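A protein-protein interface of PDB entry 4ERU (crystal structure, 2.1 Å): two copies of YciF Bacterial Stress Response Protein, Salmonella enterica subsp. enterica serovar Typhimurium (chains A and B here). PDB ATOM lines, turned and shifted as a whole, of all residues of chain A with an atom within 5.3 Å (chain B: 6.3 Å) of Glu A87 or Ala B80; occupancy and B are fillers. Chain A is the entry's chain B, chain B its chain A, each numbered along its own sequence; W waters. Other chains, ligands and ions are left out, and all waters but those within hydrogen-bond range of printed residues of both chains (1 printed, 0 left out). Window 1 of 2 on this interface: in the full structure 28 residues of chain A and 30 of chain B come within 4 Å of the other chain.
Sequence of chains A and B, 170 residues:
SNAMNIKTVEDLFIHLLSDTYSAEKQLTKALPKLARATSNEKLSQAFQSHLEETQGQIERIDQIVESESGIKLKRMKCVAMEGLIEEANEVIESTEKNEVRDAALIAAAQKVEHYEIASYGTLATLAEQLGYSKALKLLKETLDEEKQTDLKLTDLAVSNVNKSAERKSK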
ATOM      1  N   GLU A  82      31.097 -23.264 -20.695  1.00  0.00           N
ATOM      2  CA  GLU A  82      32.215 -23.221 -19.769  1.00  0.00           C
ATOM      3  C   GLU A  82      31.783 -22.633 -18.418  1.00  0.00           C
ATOM      4  O   GLU A  82      32.101 -23.194 -17.369  1.00  0.00           O
ATOM      5  CB  GLU A  82      33.380 -22.426 -20.354  1.00  0.00           C
ATOM      6  CG  GLU A  82      34.615 -22.465 -19.472  1.00  0.00           C
ATOM      7  CD  GLU A  82      35.736 -21.580 -20.017  1.00  0.00           C
ATOM      8  OE1 GLU A  82      35.427 -20.584 -20.699  1.00  0.00           O
ATOM      9  OE2 GLU A  82      36.925 -21.888 -19.774  1.00  0.00           O
ATOM     10  N   GLY A  83      31.084 -21.503 -18.459  1.00  0.00           N
ATOM     11  CA  GLY A  83      30.547 -20.879 -17.248  1.00  0.00           C
ATOM     12  C   GLY A  83      29.504 -21.737 -16.534  1.00  0.00           C
ATOM     13  O   GLY A  83      29.541 -21.868 -15.315  1.00  0.00           O
ATOM     14  N   LEU A  84      28.570 -22.335 -17.276  1.00  0.00           N
ATOM     15  CA  LEU A  84      27.617 -23.294 -16.642  1.00  0.00           C
ATOM     16  C   LEU A  84      28.296 -24.443 -15.906  1.00  0.00           C
ATOM     17  O   LEU A  84      27.880 -24.842 -14.820  1.00  0.00           O
ATOM     18  CB  LEU A  84      26.636 -23.859 -17.664  1.00  0.00           C
ATOM     19  CG  LEU A  84      25.725 -22.815 -18.285  1.00  0.00           C
ATOM     20  CD1 LEU A  84      24.725 -23.439 -19.255  1.00  0.00           C
ATOM     21  CD2 LEU A  84      25.033 -22.001 -17.198  1.00  0.00           C
ATOM     22  N   ILE A  85      29.343 -24.987 -16.494  1.00  0.00           N
ATOM     23  CA  ILE A  85      30.057 -26.070 -15.833  1.00  0.00           C
ATOM     24  C   ILE A  85      30.772 -25.561 -14.571  1.00  0.00           C
ATOM     25  O   ILE A  85      30.749 -26.223 -13.535  1.00  0.00           O
ATOM     26  CB  ILE A  85      31.011 -26.795 -16.819  1.00  0.00           C
ATOM     27  CG1 ILE A  85      30.145 -27.619 -17.802  1.00  0.00           C
ATOM     28  CG2 ILE A  85      32.064 -27.674 -16.051  1.00  0.00           C
ATOM     29  CD1 ILE A  85      30.844 -28.130 -19.045  1.00  0.00           C
ATOM     30  N   GLU A  86      31.388 -24.381 -14.652  1.00  0.00           N
ATOM     31  CA  GLU A  86      32.067 -23.805 -13.484  1.00  0.00           C
ATOM     32  C   GLU A  86      31.104 -23.537 -12.317  1.00  0.00           C
ATOM     33  O   GLU A  86      31.485 -23.675 -11.173  1.00  0.00           O
ATOM     34  CB  GLU A  86      32.809 -22.510 -13.857  1.00  0.00           C
ATOM     35  CG  GLU A  86      34.217 -22.708 -14.385  1.00  0.00           C
ATOM     36  CD  GLU A  86      34.747 -21.508 -15.245  1.00  0.00           C
ATOM     37  OE1 GLU A  86      34.050 -20.453 -15.387  1.00  0.00           O
ATOM     38  OE2 GLU A  86      35.874 -21.635 -15.801  1.00  0.00           O
ATOM     39  N   GLU A  87      29.872 -23.137 -12.625  1.00  0.00           N
ATOM     40  CA  GLU A  87      28.856 -22.925 -11.607  1.00  0.00           C
ATOM     41  C   GLU A  87      28.490 -24.237 -10.920  1.00  0.00           C
ATOM     42  O   GLU A  87      28.292 -24.263  -9.709  1.00  0.00           O
ATOM     43  CB  GLU A  87      27.617 -22.279 -12.215  1.00  0.00           C
ATOM     44  CG  GLU A  87      27.834 -20.829 -12.638  1.00  0.00           C
ATOM     45  CD  GLU A  87      26.563 -20.192 -13.165  1.00  0.00           C
ATOM     46  OE1 GLU A  87      25.454 -20.725 -12.905  1.00  0.00           O
ATOM     47  OE2 GLU A  87      26.672 -19.168 -13.850  1.00  0.00           O
ATOM     48  N   ALA A  88      28.433 -25.326 -11.688  1.00  0.00           N
ATOM     49  CA  ALA A  88      28.214 -26.654 -11.113  1.00  0.00           C
ATOM     50  C   ALA A  88      29.376 -27.003 -10.197  1.00  0.00           C
ATOM     51  O   ALA A  88      29.147 -27.494  -9.087  1.00  0.00           O
ATOM     52  CB  ALA A  88      28.016 -27.722 -12.180  1.00  0.00           C
ATOM     53  N   ASN A  89      30.611 -26.717 -10.632  1.00  0.00           N
ATOM     54  CA  ASN A  89      31.783 -27.012  -9.791  1.00  0.00           C
ATOM     55  C   ASN A  89      31.857 -26.148  -8.531  1.00  0.00           C
ATOM     56  O   ASN A  89      32.347 -26.603  -7.487  1.00  0.00           O
ATOM     57  CB  ASN A  89      33.084 -26.991 -10.598  1.00  0.00           C
ATOM     58  CG  ASN A  89      33.150 -28.130 -11.608  1.00  0.00           C
ATOM     59  OD1 ASN A  89      32.548 -29.193 -11.416  1.00  0.00           O
ATOM     60  ND2 ASN A  89      33.871 -27.908 -12.702  1.00  0.00           N
ATOM     61  N   GLU A  90      31.324 -24.931  -8.622  1.00  0.00           N
ATOM     62  CA  GLU A  90      31.214 -24.083  -7.457  1.00  0.00           C
ATOM     63  C   GLU A  90      30.176 -24.625  -6.456  1.00  0.00           C
ATOM     64  O   GLU A  90      30.381 -24.535  -5.253  1.00  0.00           O
ATOM     65  CB  GLU A  90      30.933 -22.622  -7.831  1.00  0.00           C
ATOM     66  CG  GLU A  90      31.338 -21.681  -6.698  1.00  0.00           C
ATOM     67  CD  GLU A  90      30.864 -20.228  -6.862  1.00  0.00           C
ATOM     68  OE1 GLU A  90      30.563 -19.805  -8.008  1.00  0.00           O
ATOM     69  OE2 GLU A  90      30.807 -19.508  -5.825  1.00  0.00           O
ATOM     70  N   VAL A  91      29.071 -25.191  -6.953  1.00  0.00           N
ATOM     71  CA  VAL A  91      28.137 -25.922  -6.094  1.00  0.00           C
ATOM     72  C   VAL A  91      28.872 -26.984  -5.262  1.00  0.00           C
ATOM     73  O   VAL A  91      28.741 -27.002  -4.048  1.00  0.00           O
ATOM     74  CB  VAL A  91      26.992 -26.601  -6.904  1.00  0.00           C
ATOM     75  CG1 VAL A  91      26.230 -27.595  -6.032  1.00  0.00           C
ATOM     76  CG2 VAL A  91      26.041 -25.536  -7.507  1.00  0.00           C
ATOM     77  N   ALA A 108      21.837 -26.876 -11.485  1.00  0.00           N
ATOM     78  CA  ALA A 108      22.948 -26.523 -12.398  1.00  0.00           C
ATOM     79  C   ALA A 108      22.901 -27.313 -13.729  1.00  0.00           C
ATOM     80  O   ALA A 108      23.084 -26.755 -14.826  1.00  0.00           O
ATOM     81  CB  ALA A 108      24.315 -26.762 -11.680  1.00  0.00           C
ATOM     82  N   LYS A 111      20.046 -26.117 -16.094  1.00  0.00           N
ATOM     83  CA  LYS A 111      20.527 -24.967 -16.900  1.00  0.00           C
ATOM     84  C   LYS A 111      21.410 -25.417 -18.061  1.00  0.00           C
ATOM     85  O   LYS A 111      21.228 -24.945 -19.177  1.00  0.00           O
ATOM     86  CB  LYS A 111      21.269 -23.938 -16.049  1.00  0.00           C
ATOM     87  CG  LYS A 111      20.398 -23.235 -15.009  1.00  0.00           C
ATOM     88  CD  LYS A 111      21.268 -22.446 -14.005  1.00  0.00           C
ATOM     89  CE  LYS A 111      20.428 -21.485 -13.117  1.00  0.00           C
ATOM     90  NZ  LYS A 111      19.665 -22.247 -12.078  1.00  0.00           N
ATOM     91  N   MET B   4      29.037 -18.305  -2.622  1.00  0.00           N
ATOM     92  CA  MET B   4      27.703 -18.802  -2.290  1.00  0.00           C
ATOM     93  C   MET B   4      27.955 -19.677  -1.061  1.00  0.00           C
ATOM     94  O   MET B   4      29.027 -20.291  -0.958  1.00  0.00           O
ATOM     95  CB  MET B   4      27.068 -19.606  -3.459  1.00  0.00           C
ATOM     96  CG  MET B   4      27.951 -20.696  -4.120  1.00  0.00           C
ATOM     97  SD  MET B   4      27.184 -21.827  -5.578  1.00  0.00           S
ATOM     98  CE  MET B   4      26.239 -23.142  -4.523  1.00  0.00           C
ATOM     99  N   ASP B  19      19.808 -14.939  -7.720  1.00  0.00           N
ATOM    100  CA  ASP B  19      20.469 -15.052  -9.019  1.00  0.00           C
ATOM    101  C   ASP B  19      19.465 -14.675 -10.136  1.00  0.00           C
ATOM    102  O   ASP B  19      19.777 -13.883 -11.034  1.00  0.00           O
ATOM    103  CB  ASP B  19      20.943 -16.515  -9.181  1.00  0.00           C
ATOM    104  CG  ASP B  19      21.599 -16.809 -10.536  1.00  0.00           C
ATOM    105  OD1 ASP B  19      22.811 -16.521 -10.690  1.00  0.00           O
ATOM    106  OD2 ASP B  19      20.912 -17.383 -11.441  1.00  0.00           O
ATOM    107  N   LYS B  77      25.557 -10.609  -8.709  1.00  0.00           N
ATOM    108  CA  LYS B  77      25.488 -10.524 -10.161  1.00  0.00           C
ATOM    109  C   LYS B  77      25.372 -11.928 -10.764  1.00  0.00           C
ATOM    110  O   LYS B  77      26.235 -12.781 -10.522  1.00  0.00           O
ATOM    111  CB  LYS B  77      26.701  -9.769 -10.743  1.00  0.00           C
ATOM    112  CG  LYS B  77      26.586  -9.538 -12.266  1.00  0.00           C
ATOM    113  CD  LYS B  77      27.491  -8.398 -12.739  1.00  0.00           C
ATOM    114  CE  LYS B  77      26.846  -7.616 -13.903  1.00  0.00           C
ATOM    115  NZ  LYS B  77      25.585  -6.906 -13.476  1.00  0.00           N
ATOM    116  N   CYS B  78      24.305 -12.160 -11.536  1.00  0.00           N
ATOM    117  CA  CYS B  78      24.126 -13.440 -12.220  1.00  0.00           C
ATOM    118  C   CYS B  78      25.060 -13.501 -13.429  1.00  0.00           C
ATOM    119  O   CYS B  78      24.802 -12.848 -14.453  1.00  0.00           O
ATOM    120  CB  CYS B  78      22.677 -13.630 -12.664  1.00  0.00           C
ATOM    121  SG  CYS B  78      22.457 -15.131 -13.713  1.00  0.00           S
ATOM    122  N   VAL B  79      26.130 -14.285 -13.306  1.00  0.00           N
ATOM    123  CA  VAL B  79      27.242 -14.228 -14.265  1.00  0.00           C
ATOM    124  C   VAL B  79      26.865 -14.921 -15.580  1.00  0.00           C
ATOM    125  O   VAL B  79      27.289 -14.488 -16.652  1.00  0.00           O
ATOM    126  CB  VAL B  79      28.612 -14.740 -13.647  1.00  0.00           C
ATOM    127  CG1 VAL B  79      29.671 -14.982 -14.727  1.00  0.00           C
ATOM    128  CG2 VAL B  79      29.153 -13.725 -12.593  1.00  0.00           C
ATOM    129  N   ALA B  80      26.072 -15.993 -15.491  1.00  0.00           N
ATOM    130  CA  ALA B  80      25.563 -16.663 -16.690  1.00  0.00           C
ATOM    131  C   ALA B  80      24.704 -15.718 -17.541  1.00  0.00           C
ATOM    132  O   ALA B  80      24.923 -15.579 -18.736  1.00  0.00           O
ATOM    133  CB  ALA B  80      24.768 -17.906 -16.310  1.00  0.00           C
ATOM    134  N   MET B  81      23.737 -15.049 -16.925  1.00  0.00           N
ATOM    135  CA  MET B  81      22.951 -14.118 -17.693  1.00  0.00           C
ATOM    136  C   MET B  81      23.861 -13.052 -18.278  1.00  0.00           C
ATOM    137  O   MET B  81      23.664 -12.637 -19.409  1.00  0.00           O
ATOM    138  CB  MET B  81      21.832 -13.469 -16.852  1.00  0.00           C
ATOM    139  CG  MET B  81      20.980 -12.459 -17.673  1.00  0.00           C
ATOM    140  SD  MET B  81      20.121 -13.342 -19.198  1.00  0.00           S
ATOM    141  CE  MET B  81      18.901 -14.585 -18.237  1.00  0.00           C
ATOM    142  N   GLU B  82      24.855 -12.603 -17.516  1.00  0.00           N
ATOM    143  CA  GLU B  82      25.774 -11.600 -18.040  1.00  0.00           C
ATOM    144  C   GLU B  82      26.449 -12.076 -19.314  1.00  0.00           C
ATOM    145  O   GLU B  82      26.566 -11.308 -20.288  1.00  0.00           O
ATOM    146  CB  GLU B  82      26.817 -11.179 -16.978  1.00  0.00           C
ATOM    147  CG  GLU B  82      27.689  -9.999 -17.412  1.00  0.00           C
ATOM    148  CD  GLU B  82      28.724  -9.620 -16.353  1.00  0.00           C
ATOM    149  OE1 GLU B  82      29.285 -10.528 -15.702  1.00  0.00           O
ATOM    150  OE2 GLU B  82      28.975  -8.408 -16.178  1.00  0.00           O
ATOM    151  N   GLY B  83      26.906 -13.323 -19.311  1.00  0.00           N
ATOM    152  CA  GLY B  83      27.578 -13.896 -20.493  1.00  0.00           C
ATOM    153  C   GLY B  83      26.594 -14.053 -21.661  1.00  0.00           C
ATOM    154  O   GLY B  83      26.937 -13.748 -22.813  1.00  0.00           O
ATOM    155  N   LEU B  84      25.365 -14.512 -21.374  1.00  0.00           N
ATOM    156  CA  LEU B  84      24.341 -14.630 -22.451  1.00  0.00           C
ATOM    157  C   LEU B  84      23.995 -13.294 -23.094  1.00  0.00           C
ATOM    158  O   LEU B  84      23.869 -13.185 -24.333  1.00  0.00           O
ATOM    159  CB  LEU B  84      23.075 -15.353 -21.950  1.00  0.00           C
ATOM    160  CG  LEU B  84      23.287 -16.813 -21.503  1.00  0.00           C
ATOM    161  CD1 LEU B  84      21.988 -17.481 -20.987  1.00  0.00           C
ATOM    162  CD2 LEU B  84      23.915 -17.677 -22.627  1.00  0.00           C
ATOM    163  N   ILE B  85      23.879 -12.255 -22.278  1.00  0.00           N
ATOM    164  CA  ILE B  85      23.663 -10.913 -22.825  1.00  0.00           C
ATOM    165  C   ILE B  85      24.869 -10.407 -23.629  1.00  0.00           C
ATOM    166  O   ILE B  85      24.692  -9.775 -24.658  1.00  0.00           O
ATOM    167  CB  ILE B  85      23.262  -9.890 -21.716  1.00  0.00           C
ATOM    168  CG1 ILE B  85      21.889 -10.268 -21.153  1.00  0.00           C
ATOM    169  CG2 ILE B  85      23.187  -8.467 -22.288  1.00  0.00           C
ATOM    170  CD1 ILE B  85      21.484  -9.584 -19.869  1.00  0.00           C
ATOM    171  N   TYR B 115      17.564 -20.404 -20.051  1.00  0.00           N
ATOM    172  CA  TYR B 115      18.232 -20.242 -18.770  1.00  0.00           C
ATOM    173  C   TYR B 115      17.160 -19.923 -17.701  1.00  0.00           C
ATOM    174  O   TYR B 115      17.194 -20.443 -16.561  1.00  0.00           O
ATOM    175  CB  TYR B 115      19.248 -19.095 -18.833  1.00  0.00           C
ATOM    176  CG  TYR B 115      19.954 -18.875 -17.492  1.00  0.00           C
ATOM    177  CD1 TYR B 115      21.098 -19.614 -17.161  1.00  0.00           C
ATOM    178  CD2 TYR B 115      19.468 -17.938 -16.550  1.00  0.00           C
ATOM    179  CE1 TYR B 115      21.746 -19.439 -15.929  1.00  0.00           C
ATOM    180  CE2 TYR B 115      20.118 -17.767 -15.305  1.00  0.00           C
ATOM    181  CZ  TYR B 115      21.233 -18.525 -15.015  1.00  0.00           C
ATOM    182  OH  TYR B 115      21.887 -18.351 -13.829  1.00  0.00           O
HETATM  183  O   HOH W   1      18.836 -19.385 -10.691  1.00  0.00           O
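The side-chain hydroxyl of Tyr B115 is in hydrogen-bond range of the side-chain carboxylate of Asp B19 (2.8 Å). SG of Cys B78 lies within hydrogen-bond range of OH of Tyr B115 (3.3 Å).
Glu A87 touches Ala B80. Met B4 touches Glu A90. CA of Val A91 touches CE of Met B4, 3.7 Å away. CE of Lys A111 touches OH of Tyr B115 (3.5 Å).
Printed residues of chain A within 4 Å of Ala B80: Glu A87. Of the printed residues of chain A, Met B4 touches Glu A90 (3.5 Å) and Val A91 (3.7 Å). Printed residues of chain A within 4 Å of Tyr B115: Lys A111 (3.5 Å). Printed residues of chain B within 4 Å of Val A91: Met B4 (3.7 Å). Printed residues of chain B within 4 Å of Lys A111: Tyr B115. Of the printed residues of chain B, Glu A90 touches Met B4. Ile B85 touches none of the printed residues of chain A. Glu A86 touches none of the printed residues of chain B. The nearest printed residue of chain A that does not touch Ala B80 is Leu A84 (4.2 Å). The nearest printed residue of chain B that does not touch Lys A111 is Asp B19 (4.5 Å).
Printed residues of chain A that touch a printed residue of chain B: Glu A87, Glu A90, Val A91 and Lys A111. Hydrophobic or aromatic side chains of chain A within 4 Å of the printed part of chain B: Val A91. Along chain A the printed residues that touch a printed residue of chain B span positions 87 to 111. Hydrophobic or aromatic side chains of chain B that line the printed part of chain A: Met B4, Ala B80 and Tyr B115. Among the printed residues, 4 pairs touch across the chains. Among the printed residues, no Asp or Glu carboxylate lies within 4 Å of a Lys or Arg side-chain nitrogen of the other chain.
4 positions are printed for both chains. Of the 4 pairs that touch across the chains among the printed residues, none has its exchanged pair printed and touching as well.
Water W1 lies within hydrogen-bond range of OD2 of Asp B19 (3.0 Å) and NZ of Lys A111 (3.3 Å).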
